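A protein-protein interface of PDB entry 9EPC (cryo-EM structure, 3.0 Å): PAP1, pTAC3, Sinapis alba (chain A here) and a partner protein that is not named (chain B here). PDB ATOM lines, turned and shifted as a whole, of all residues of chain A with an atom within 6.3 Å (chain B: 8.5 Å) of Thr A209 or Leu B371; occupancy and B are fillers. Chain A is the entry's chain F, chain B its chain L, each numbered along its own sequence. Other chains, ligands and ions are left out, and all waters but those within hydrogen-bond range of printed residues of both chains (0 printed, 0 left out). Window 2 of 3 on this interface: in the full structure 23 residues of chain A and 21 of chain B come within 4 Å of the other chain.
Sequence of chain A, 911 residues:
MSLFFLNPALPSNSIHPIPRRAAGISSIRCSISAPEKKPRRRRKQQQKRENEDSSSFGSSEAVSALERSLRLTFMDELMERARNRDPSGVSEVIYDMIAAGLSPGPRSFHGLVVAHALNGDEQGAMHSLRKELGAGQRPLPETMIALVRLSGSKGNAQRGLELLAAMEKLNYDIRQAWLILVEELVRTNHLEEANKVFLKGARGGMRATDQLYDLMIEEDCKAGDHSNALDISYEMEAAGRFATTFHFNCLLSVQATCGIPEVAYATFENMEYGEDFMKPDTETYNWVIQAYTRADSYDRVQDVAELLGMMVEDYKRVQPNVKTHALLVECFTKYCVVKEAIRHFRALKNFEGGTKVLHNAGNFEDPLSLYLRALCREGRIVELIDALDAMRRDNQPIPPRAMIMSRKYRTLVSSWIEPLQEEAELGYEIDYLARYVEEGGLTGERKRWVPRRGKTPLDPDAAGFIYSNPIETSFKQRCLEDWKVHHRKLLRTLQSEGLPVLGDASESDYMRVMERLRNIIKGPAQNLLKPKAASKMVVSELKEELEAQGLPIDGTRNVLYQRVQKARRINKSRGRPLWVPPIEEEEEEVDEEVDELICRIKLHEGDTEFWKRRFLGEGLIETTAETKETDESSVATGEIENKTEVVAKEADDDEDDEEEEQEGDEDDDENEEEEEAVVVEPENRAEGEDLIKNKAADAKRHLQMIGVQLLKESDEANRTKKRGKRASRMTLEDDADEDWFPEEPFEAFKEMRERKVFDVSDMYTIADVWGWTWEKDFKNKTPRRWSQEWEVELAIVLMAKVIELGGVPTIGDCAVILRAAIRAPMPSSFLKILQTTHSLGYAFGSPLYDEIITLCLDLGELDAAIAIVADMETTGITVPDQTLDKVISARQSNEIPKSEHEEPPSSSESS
Of the 14 printed residues of chain B, 4 touch a printed residue of chain A. Hydrophobic or aromatic side chains of chain B within 4 Å of the printed part of chain A: Phe B369, Leu B371 and Tyr B376. Of the 14 printed residues of chain A, 5 touch a printed residue of chain B. Printed residues of chain A that touch a printed residue of chain B: Asp A173, Arg A175, Gln A176, Leu A179 and Thr A209. Hydrophobic or aromatic side chains of chain A within 4 Å of the printed part of chain B: Leu A179. Among the printed residues, 8 pairs touch across the chains. Among the printed residues, no Asp or Glu carboxylate lies within 4 Å of a Lys or Arg side-chain nitrogen of the other chain.
OD2 of Asp A173 sits at hydrogen-bond distance from OH of Tyr B376 (3.1 Å). N of Gly B370 lies within hydrogen-bond range of OE1 of Gln A176 (2.9 Å). N of Gly B370 sits at hydrogen-bond distance from OD2 of Asp A173, 3.4 Å away.
Asp A173 touches Phe B369 (OD2 to CB, 3.6 Å). Arg A175 touches Leu B371 (NH1 to CD1, 3.4 Å). Gln A176 touches Leu B371. Leu B371 touches Leu A179. Leu B371 touches Thr A209 (CD2 to CG2, 3.7 Å).
Of the printed residues of chain B, Asp A173 touches Phe B369, Gly B370 and Tyr B376. Printed residues of chain B within 4 Å of Arg A175: Leu B371 (3.4 Å). Printed residues of chain B within 4 Å of Leu A179: Leu B371. Ala A208 touches none of the printed residues of chain B. Thr A209 touches just one residue of chain B: Leu B371 (3.7 Å). Asp A210 touches none of the printed residues of chain B. Tyr B375 touches none of the printed residues of chain A. Of the printed residues of chain A, Tyr B376 touches Asp A173.
The backbone NH (N) of Phe B369 sits at hydrogen-bond distance from the backbone carbonyl oxygen (O) of Tyr B376 (3.1 Å). OG1 of Thr A209 lies within hydrogen-bond range of N of Leu A212, 3.2 Å away. The backbone NH of Arg A175 lies close to the side-chain carboxylate of Asp A173 (3.2 Å). NE of Arg A175 sits at hydrogen-bond distance from O of Arg A207 (2.6 Å).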
ATOM      1  N   ASP A 173     -32.357   8.221  19.418  1.00  0.00           N
ATOM      2  CA  ASP A 173     -31.935   6.925  19.950  1.00  0.00           C
ATOM      3  C   ASP A 173     -32.065   6.979  21.466  1.00  0.00           C
ATOM      4  O   ASP A 173     -31.150   7.393  22.178  1.00  0.00           O
ATOM      5  CB  ASP A 173     -30.512   6.599  19.516  1.00  0.00           C
ATOM      6  CG  ASP A 173     -30.144   5.143  19.750  1.00  0.00           C
ATOM      7  OD1 ASP A 173     -30.777   4.489  20.605  1.00  0.00           O
ATOM      8  OD2 ASP A 173     -29.215   4.650  19.076  1.00  0.00           O
ATOM      9  N   ARG A 175     -32.199   4.509  23.477  1.00  0.00           N
ATOM     10  CA  ARG A 175     -31.501   3.425  24.162  1.00  0.00           C
ATOM     11  C   ARG A 175     -30.196   3.903  24.786  1.00  0.00           C
ATOM     12  O   ARG A 175     -29.925   3.636  25.963  1.00  0.00           O
ATOM     13  CB  ARG A 175     -31.236   2.279  23.187  1.00  0.00           C
ATOM     14  CG  ARG A 175     -30.300   1.219  23.735  1.00  0.00           C
ATOM     15  CD  ARG A 175     -30.026   0.135  22.711  1.00  0.00           C
ATOM     16  NE  ARG A 175     -29.090  -0.858  23.221  1.00  0.00           N
ATOM     17  CZ  ARG A 175     -27.775  -0.784  23.087  1.00  0.00           C
ATOM     18  NH1 ARG A 175     -27.202   0.223  22.449  1.00  0.00           N
ATOM     19  NH2 ARG A 175     -27.013  -1.743  23.605  1.00  0.00           N
ATOM     20  N   GLN A 176     -29.373   4.616  24.014  1.00  0.00           N
ATOM     21  CA  GLN A 176     -28.073   5.041  24.525  1.00  0.00           C
ATOM     22  C   GLN A 176     -28.226   5.989  25.707  1.00  0.00           C
ATOM     23  O   GLN A 176     -27.480   5.896  26.688  1.00  0.00           O
ATOM     24  CB  GLN A 176     -27.256   5.693  23.411  1.00  0.00           C
ATOM     25  CG  GLN A 176     -25.811   5.960  23.791  1.00  0.00           C
ATOM     26  CD  GLN A 176     -24.979   6.424  22.615  1.00  0.00           C
ATOM     27  OE1 GLN A 176     -25.513   6.842  21.587  1.00  0.00           O
ATOM     28  NE2 GLN A 176     -23.661   6.348  22.756  1.00  0.00           N
ATOM     29  N   TRP A 178     -30.892   5.980  27.609  1.00  0.00           N
ATOM     30  CA  TRP A 178     -31.502   5.161  28.651  1.00  0.00           C
ATOM     31  C   TRP A 178     -30.454   4.404  29.455  1.00  0.00           C
ATOM     32  O   TRP A 178     -30.622   4.212  30.665  1.00  0.00           O
ATOM     33  CB  TRP A 178     -32.507   4.193  28.026  1.00  0.00           C
ATOM     34  CG  TRP A 178     -33.015   3.147  28.961  1.00  0.00           C
ATOM     35  CD1 TRP A 178     -33.910   3.317  29.974  1.00  0.00           C
ATOM     36  CD2 TRP A 178     -32.671   1.757  28.958  1.00  0.00           C
ATOM     37  NE1 TRP A 178     -34.139   2.122  30.609  1.00  0.00           N
ATOM     38  CE2 TRP A 178     -33.390   1.148  30.003  1.00  0.00           C
ATOM     39  CE3 TRP A 178     -31.822   0.971  28.176  1.00  0.00           C
ATOM     40  CZ2 TRP A 178     -33.286  -0.211  30.286  1.00  0.00           C
ATOM     41  CZ3 TRP A 178     -31.721  -0.377  28.458  1.00  0.00           C
ATOM     42  CH2 TRP A 178     -32.448  -0.954  29.504  1.00  0.00           C
ATOM     43  N   LEU A 179     -29.374   3.963  28.806  1.00  0.00           N
ATOM     44  CA  LEU A 179     -28.302   3.293  29.533  1.00  0.00           C
ATOM     45  C   LEU A 179     -27.651   4.228  30.543  1.00  0.00           C
ATOM     46  O   LEU A 179     -27.376   3.832  31.681  1.00  0.00           O
ATOM     47  CB  LEU A 179     -27.255   2.765  28.552  1.00  0.00           C
ATOM     48  CG  LEU A 179     -27.743   1.837  27.443  1.00  0.00           C
ATOM     49  CD1 LEU A 179     -26.617   1.543  26.470  1.00  0.00           C
ATOM     50  CD2 LEU A 179     -28.294   0.552  28.024  1.00  0.00           C
ATOM     51  N   ARG A 207     -32.038  -3.677  24.288  1.00  0.00           N
ATOM     52  CA  ARG A 207     -31.081  -4.512  25.001  1.00  0.00           C
ATOM     53  C   ARG A 207     -30.017  -3.636  25.646  1.00  0.00           C
ATOM     54  O   ARG A 207     -29.402  -2.802  24.976  1.00  0.00           O
ATOM     55  CB  ARG A 207     -30.424  -5.522  24.060  1.00  0.00           C
ATOM     56  CG  ARG A 207     -29.497  -6.497  24.767  1.00  0.00           C
ATOM     57  CD  ARG A 207     -28.243  -6.771  23.957  1.00  0.00           C
ATOM     58  NE  ARG A 207     -27.325  -7.651  24.669  1.00  0.00           N
ATOM     59  CZ  ARG A 207     -26.081  -7.903  24.287  1.00  0.00           C
ATOM     60  NH1 ARG A 207     -25.563  -7.346  23.206  1.00  0.00           N
ATOM     61  NH2 ARG A 207     -25.334  -8.731  25.014  1.00  0.00           N
ATOM     62  N   ALA A 208     -29.807  -3.829  26.943  1.00  0.00           N
ATOM     63  CA  ALA A 208     -28.770  -3.101  27.651  1.00  0.00           C
ATOM     64  C   ALA A 208     -27.400  -3.699  27.344  1.00  0.00           C
ATOM     65  O   ALA A 208     -27.275  -4.772  26.747  1.00  0.00           O
ATOM     66  CB  ALA A 208     -29.035  -3.117  29.155  1.00  0.00           C
ATOM     67  N   THR A 209     -26.359  -2.983  27.754  1.00  0.00           N
ATOM     68  CA  THR A 209     -25.005  -3.475  27.568  1.00  0.00           C
ATOM     69  C   THR A 209     -24.718  -4.620  28.533  1.00  0.00           C
ATOM     70  O   THR A 209     -25.417  -4.822  29.529  1.00  0.00           O
ATOM     71  CB  THR A 209     -23.987  -2.354  27.773  1.00  0.00           C
ATOM     72  OG1 THR A 209     -24.102  -1.841  29.105  1.00  0.00           O
ATOM     73  CG2 THR A 209     -24.230  -1.232  26.782  1.00  0.00           C
ATOM     74  N   ASP A 210     -23.665  -5.379  28.221  1.00  0.00           N
ATOM     75  CA  ASP A 210     -23.272  -6.485  29.087  1.00  0.00           C
ATOM     76  C   ASP A 210     -22.869  -5.984  30.467  1.00  0.00           C
ATOM     77  O   ASP A 210     -23.204  -6.604  31.484  1.00  0.00           O
ATOM     78  CB  ASP A 210     -22.131  -7.273  28.447  1.00  0.00           C
ATOM     79  CG  ASP A 210     -22.541  -7.935  27.148  1.00  0.00           C
ATOM     80  OD1 ASP A 210     -23.714  -8.348  27.036  1.00  0.00           O
ATOM     81  OD2 ASP A 210     -21.690  -8.041  26.240  1.00  0.00           O
ATOM     82  N   GLN A 211     -22.144  -4.865  30.522  1.00  0.00           N
ATOM     83  CA  GLN A 211     -21.746  -4.305  31.809  1.00  0.00           C
ATOM     84  C   GLN A 211     -22.961  -3.888  32.626  1.00  0.00           C
ATOM     85  O   GLN A 211     -23.009  -4.117  33.840  1.00  0.00           O
ATOM     86  CB  GLN A 211     -20.813  -3.111  31.602  1.00  0.00           C
ATOM     87  CG  GLN A 211     -19.524  -3.433  30.862  1.00  0.00           C
ATOM     88  CD  GLN A 211     -19.708  -3.500  29.358  1.00  0.00           C
ATOM     89  OE1 GLN A 211     -20.818  -3.344  28.849  1.00  0.00           O
ATOM     90  NE2 GLN A 211     -18.616  -3.730  28.639  1.00  0.00           N
ATOM     91  N   LEU A 212     -23.951  -3.272  31.978  1.00  0.00           N
ATOM     92  CA  LEU A 212     -25.126  -2.805  32.705  1.00  0.00           C
ATOM     93  C   LEU A 212     -25.891  -3.966  33.325  1.00  0.00           C
ATOM     94  O   LEU A 212     -26.334  -3.879  34.476  1.00  0.00           O
ATOM     95  CB  LEU A 212     -26.032  -1.993  31.781  1.00  0.00           C
ATOM     96  CG  LEU A 212     -27.254  -1.377  32.463  1.00  0.00           C
ATOM     97  CD1 LEU A 212     -26.843  -0.623  33.715  1.00  0.00           C
ATOM     98  CD2 LEU A 212     -27.994  -0.458  31.512  1.00  0.00           C
ATOM     99  N   TYR A 213     -26.058  -5.062  32.582  1.00  0.00           N
ATOM    100  CA  TYR A 213     -26.715  -6.237  33.146  1.00  0.00           C
ATOM    101  C   TYR A 213     -25.936  -6.776  34.337  1.00  0.00           C
ATOM    102  O   TYR A 213     -26.517  -7.099  35.380  1.00  0.00           O
ATOM    103  CB  TYR A 213     -26.875  -7.322  32.080  1.00  0.00           C
ATOM    104  CG  TYR A 213     -27.971  -7.058  31.076  1.00  0.00           C
ATOM    105  CD1 TYR A 213     -29.296  -6.965  31.476  1.00  0.00           C
ATOM    106  CD2 TYR A 213     -27.684  -6.923  29.726  1.00  0.00           C
ATOM    107  CE1 TYR A 213     -30.301  -6.731  30.561  1.00  0.00           C
ATOM    108  CE2 TYR A 213     -28.683  -6.691  28.805  1.00  0.00           C
ATOM    109  CZ  TYR A 213     -29.989  -6.595  29.228  1.00  0.00           C
ATOM    110  OH  TYR A 213     -30.988  -6.363  28.312  1.00  0.00           O
ATOM    111  N   ASP A 214     -24.612  -6.878  34.201  1.00  0.00           N
ATOM    112  CA  ASP A 214     -23.791  -7.347  35.312  1.00  0.00           C
ATOM    113  C   ASP A 214     -23.837  -6.374  36.482  1.00  0.00           C
ATOM    114  O   ASP A 214     -23.953  -6.792  37.639  1.00  0.00           O
ATOM    115  CB  ASP A 214     -22.351  -7.554  34.847  1.00  0.00           C
ATOM    116  CG  ASP A 214     -22.248  -8.531  33.699  1.00  0.00           C
ATOM    117  OD1 ASP A 214     -23.305  -8.970  33.200  1.00  0.00           O
ATOM    118  OD2 ASP A 214     -21.114  -8.861  33.295  1.00  0.00           O
ATOM    119  N   ARG A 241     -28.905 -12.372  25.641  1.00  0.00           N
ATOM    120  CA  ARG A 241     -27.735 -12.716  26.436  1.00  0.00           C
ATOM    121  C   ARG A 241     -28.138 -13.731  27.495  1.00  0.00           C
ATOM    122  O   ARG A 241     -29.169 -13.569  28.155  1.00  0.00           O
ATOM    123  CB  ARG A 241     -27.128 -11.480  27.098  1.00  0.00           C
ATOM    124  CG  ARG A 241     -25.841 -11.773  27.844  1.00  0.00           C
ATOM    125  CD  ARG A 241     -25.449 -10.637  28.766  1.00  0.00           C
ATOM    126  NE  ARG A 241     -24.200 -10.926  29.459  1.00  0.00           N
ATOM    127  CZ  ARG A 241     -23.698 -10.189  30.438  1.00  0.00           C
ATOM    128  NH1 ARG A 241     -24.320  -9.110  30.880  1.00  0.00           N
ATOM    129  NH2 ARG A 241     -22.542 -10.547  30.991  1.00  0.00           N
ATOM    130  N   TRP B 346     -15.351   0.107   8.907  1.00  0.00           N
ATOM    131  CA  TRP B 346     -14.286  -0.388   9.762  1.00  0.00           C
ATOM    132  C   TRP B 346     -12.891  -0.085   9.238  1.00  0.00           C
ATOM    133  O   TRP B 346     -11.912  -0.450   9.896  1.00  0.00           O
ATOM    134  CB  TRP B 346     -14.435  -1.900   9.975  1.00  0.00           C
ATOM    135  CG  TRP B 346     -15.731  -2.258  10.617  1.00  0.00           C
ATOM    136  CD1 TRP B 346     -16.905  -2.543   9.986  1.00  0.00           C
ATOM    137  CD2 TRP B 346     -15.994  -2.353  12.020  1.00  0.00           C
ATOM    138  NE1 TRP B 346     -17.883  -2.816  10.910  1.00  0.00           N
ATOM    139  CE2 TRP B 346     -17.349  -2.706  12.167  1.00  0.00           C
ATOM    140  CE3 TRP B 346     -15.215  -2.178  13.167  1.00  0.00           C
ATOM    141  CZ2 TRP B 346     -17.941  -2.888  13.413  1.00  0.00           C
ATOM    142  CZ3 TRP B 346     -15.805  -2.357  14.402  1.00  0.00           C
ATOM    143  CH2 TRP B 346     -17.154  -2.709  14.517  1.00  0.00           C
ATOM    144  N   LEU B 359     -15.883  13.841  19.482  1.00  0.00           N
ATOM    145  CA  LEU B 359     -16.606  12.960  18.573  1.00  0.00           C
ATOM    146  C   LEU B 359     -18.112  13.040  18.780  1.00  0.00           C
ATOM    147  O   LEU B 359     -18.878  12.799  17.840  1.00  0.00           O
ATOM    148  CB  LEU B 359     -16.130  11.516  18.731  1.00  0.00           C
ATOM    149  CG  LEU B 359     -16.444  10.784  20.036  1.00  0.00           C
ATOM    150  CD1 LEU B 359     -16.607   9.299  19.770  1.00  0.00           C
ATOM    151  CD2 LEU B 359     -15.351  11.015  21.061  1.00  0.00           C
ATOM    152  N   LEU B 363     -20.451  12.918  15.964  1.00  0.00           N
ATOM    153  CA  LEU B 363     -21.469  11.887  15.784  1.00  0.00           C
ATOM    154  C   LEU B 363     -22.835  12.500  15.502  1.00  0.00           C
ATOM    155  O   LEU B 363     -23.561  12.041  14.613  1.00  0.00           O
ATOM    156  CB  LEU B 363     -21.531  10.989  17.019  1.00  0.00           C
ATOM    157  CG  LEU B 363     -20.342  10.060  17.269  1.00  0.00           C
ATOM    158  CD1 LEU B 363     -20.506   9.324  18.589  1.00  0.00           C
ATOM    159  CD2 LEU B 363     -20.188   9.080  16.124  1.00  0.00           C
ATOM    160  N   ILE B 368     -25.407  10.240  13.691  1.00  0.00           N
ATOM    161  CA  ILE B 368     -24.866   8.942  14.075  1.00  0.00           C
ATOM    162  C   ILE B 368     -25.123   8.744  15.560  1.00  0.00           C
ATOM    163  O   ILE B 368     -24.769   9.601  16.380  1.00  0.00           O
ATOM    164  CB  ILE B 368     -23.365   8.844  13.755  1.00  0.00           C
ATOM    165  CG1 ILE B 368     -23.119   9.109  12.270  1.00  0.00           C
ATOM    166  CG2 ILE B 368     -22.830   7.478  14.146  1.00  0.00           C
ATOM    167  CD1 ILE B 368     -21.669   8.979  11.861  1.00  0.00           C
ATOM    168  N   PHE B 369     -25.739   7.619  15.911  1.00  0.00           N
ATOM    169  CA  PHE B 369     -26.145   7.347  17.281  1.00  0.00           C
ATOM    170  C   PHE B 369     -25.686   5.951  17.682  1.00  0.00           C
ATOM    171  O   PHE B 369     -25.144   5.191  16.873  1.00  0.00           O
ATOM    172  CB  PHE B 369     -27.663   7.488  17.441  1.00  0.00           C
ATOM    173  CG  PHE B 369     -28.211   8.765  16.881  1.00  0.00           C
ATOM    174  CD1 PHE B 369     -28.184   9.931  17.626  1.00  0.00           C
ATOM    175  CD2 PHE B 369     -28.753   8.802  15.609  1.00  0.00           C
ATOM    176  CE1 PHE B 369     -28.687  11.108  17.113  1.00  0.00           C
ATOM    177  CE2 PHE B 369     -29.259   9.976  15.090  1.00  0.00           C
ATOM    178  CZ  PHE B 369     -29.226  11.132  15.843  1.00  0.00           C
ATOM    179  N   GLY B 370     -25.912   5.617  18.949  1.00  0.00           N
ATOM    180  CA  GLY B 370     -25.553   4.321  19.480  1.00  0.00           C
ATOM    181  C   GLY B 370     -24.112   4.255  19.949  1.00  0.00           C
ATOM    182  O   GLY B 370     -23.304   5.164  19.745  1.00  0.00           O
ATOM    183  N   LEU B 371     -23.790   3.139  20.595  1.00  0.00           N
ATOM    184  CA  LEU B 371     -22.440   2.904  21.068  1.00  0.00           C
ATOM    185  C   LEU B 371     -21.509   2.651  19.883  1.00  0.00           C
ATOM    186  O   LEU B 371     -21.965   2.335  18.782  1.00  0.00           O
ATOM    187  CB  LEU B 371     -22.415   1.717  22.029  1.00  0.00           C
ATOM    188  CG  LEU B 371     -22.945   1.935  23.448  1.00  0.00           C
ATOM    189  CD1 LEU B 371     -24.463   1.886  23.488  1.00  0.00           C
ATOM    190  CD2 LEU B 371     -22.347   0.914  24.403  1.00  0.00           C
ATOM    191  N   PRO B 372     -20.195   2.804  20.079  1.00  0.00           N
ATOM    192  CA  PRO B 372     -19.264   2.555  18.966  1.00  0.00           C
ATOM    193  C   PRO B 372     -19.376   1.158  18.387  1.00  0.00           C
ATOM    194  O   PRO B 372     -19.108   0.968  17.195  1.00  0.00           O
ATOM    195  CB  PRO B 372     -17.885   2.800  19.597  1.00  0.00           C
ATOM    196  CG  PRO B 372     -18.111   2.735  21.077  1.00  0.00           C
ATOM    197  CD  PRO B 372     -19.487   3.270  21.283  1.00  0.00           C
ATOM    198  N   GLU B 373     -19.765   0.171  19.195  1.00  0.00           N
ATOM    199  CA  GLU B 373     -19.995  -1.167  18.669  1.00  0.00           C
ATOM    200  C   GLU B 373     -21.222  -1.229  17.770  1.00  0.00           C
ATOM    201  O   GLU B 373     -21.359  -2.182  16.996  1.00  0.00           O
ATOM    202  CB  GLU B 373     -20.143  -2.170  19.815  1.00  0.00           C
ATOM    203  CG  GLU B 373     -18.944  -2.252  20.750  1.00  0.00           C
ATOM    204  CD  GLU B 373     -18.923  -1.142  21.785  1.00  0.00           C
ATOM    205  OE1 GLU B 373     -19.874  -0.334  21.812  1.00  0.00           O
ATOM    206  OE2 GLU B 373     -17.954  -1.078  22.570  1.00  0.00           O
ATOM    207  N   GLU B 374     -22.113  -0.243  17.852  1.00  0.00           N
ATOM    208  CA  GLU B 374     -23.348  -0.220  17.078  1.00  0.00           C
ATOM    209  C   GLU B 374     -23.556   1.141  16.430  1.00  0.00           C
ATOM    210  O   GLU B 374     -24.669   1.674  16.406  1.00  0.00           O
ATOM    211  CB  GLU B 374     -24.552  -0.579  17.947  1.00  0.00           C
ATOM    212  CG  GLU B 374     -24.472  -1.939  18.628  1.00  0.00           C
ATOM    213  CD  GLU B 374     -23.675  -1.905  19.919  1.00  0.00           C
ATOM    214  OE1 GLU B 374     -23.098  -0.844  20.236  1.00  0.00           O
ATOM    215  OE2 GLU B 374     -23.628  -2.938  20.619  1.00  0.00           O
ATOM    216  N   TYR B 375     -22.486   1.731  15.904  1.00  0.00           N
ATOM    217  CA  TYR B 375     -22.612   2.996  15.193  1.00  0.00           C
ATOM    218  C   TYR B 375     -23.476   2.821  13.951  1.00  0.00           C
ATOM    219  O   TYR B 375     -23.296   1.871  13.183  1.00  0.00           O
ATOM    220  CB  TYR B 375     -21.234   3.527  14.801  1.00  0.00           C
ATOM    221  CG  TYR B 375     -20.547   4.331  15.877  1.00  0.00           C
ATOM    222  CD1 TYR B 375     -21.272   4.920  16.903  1.00  0.00           C
ATOM    223  CD2 TYR B 375     -19.170   4.508  15.862  1.00  0.00           C
ATOM    224  CE1 TYR B 375     -20.646   5.659  17.885  1.00  0.00           C
ATOM    225  CE2 TYR B 375     -18.535   5.245  16.841  1.00  0.00           C
ATOM    226  CZ  TYR B 375     -19.277   5.818  17.849  1.00  0.00           C
ATOM    227  OH  TYR B 375     -18.648   6.553  18.828  1.00  0.00           O
ATOM    228  N   TYR B 376     -24.418   3.739  13.758  1.00  0.00           N
ATOM    229  CA  TYR B 376     -25.276   3.707  12.584  1.00  0.00           C
ATOM    230  C   TYR B 376     -25.847   5.098  12.362  1.00  0.00           C
ATOM    231  O   TYR B 376     -25.867   5.934  13.269  1.00  0.00           O
ATOM    232  CB  TYR B 376     -26.401   2.678  12.732  1.00  0.00           C
ATOM    233  CG  TYR B 376     -27.501   3.104  13.672  1.00  0.00           C
ATOM    234  CD1 TYR B 376     -27.337   3.020  15.047  1.00  0.00           C
ATOM    235  CD2 TYR B 376     -28.709   3.583  13.183  1.00  0.00           C
ATOM    236  CE1 TYR B 376     -28.342   3.408  15.910  1.00  0.00           C
ATOM    237  CE2 TYR B 376     -29.719   3.972  14.037  1.00  0.00           C
ATOM    238  CZ  TYR B 376     -29.532   3.882  15.399  1.00  0.00           C
ATOM    239  OH  TYR B 376     -30.538   4.269  16.253  1.00  0.00           O
ATOM    240  N   ILE B 393     -18.809   6.697   8.913  1.00  0.00           N
ATOM    241  CA  ILE B 393     -18.935   6.026  10.203  1.00  0.00           C
ATOM    242  C   ILE B 393     -17.583   5.498  10.660  1.00  0.00           C
ATOM    243  O   ILE B 393     -17.245   5.560  11.848  1.00  0.00           O
ATOM    244  CB  ILE B 393     -19.987   4.907  10.119  1.00  0.00           C
ATOM    245  CG1 ILE B 393     -21.347   5.489   9.732  1.00  0.00           C
ATOM    246  CG2 ILE B 393     -20.083   4.166  11.439  1.00  0.00           C
ATOM    247  CD1 ILE B 393     -22.453   4.462   9.663  1.00  0.00           C
ATOM    248  N   ARG B 397     -14.492   6.236  14.255  1.00  0.00           N
ATOM    249  CA  ARG B 397     -13.653   5.329  15.027  1.00  0.00           C
ATOM    250  C   ARG B 397     -12.166   5.590  14.824  1.00  0.00           C
ATOM    251  O   ARG B 397     -11.415   5.674  15.800  1.00  0.00           O
ATOM    252  CB  ARG B 397     -13.978   3.875  14.663  1.00  0.00           C
ATOM    253  CG  ARG B 397     -15.423   3.474  14.905  1.00  0.00           C
ATOM    254  CD  ARG B 397     -15.621   1.993  14.640  1.00  0.00           C
ATOM    255  NE  ARG B 397     -16.996   1.565  14.869  1.00  0.00           N
ATOM    256  CZ  ARG B 397     -17.925   1.497  13.926  1.00  0.00           C
ATOM    257  NH1 ARG B 397     -17.666   1.836  12.674  1.00  0.00           N
ATOM    258  NH2 ARG B 397     -19.144   1.073  14.246  1.00  0.00           N
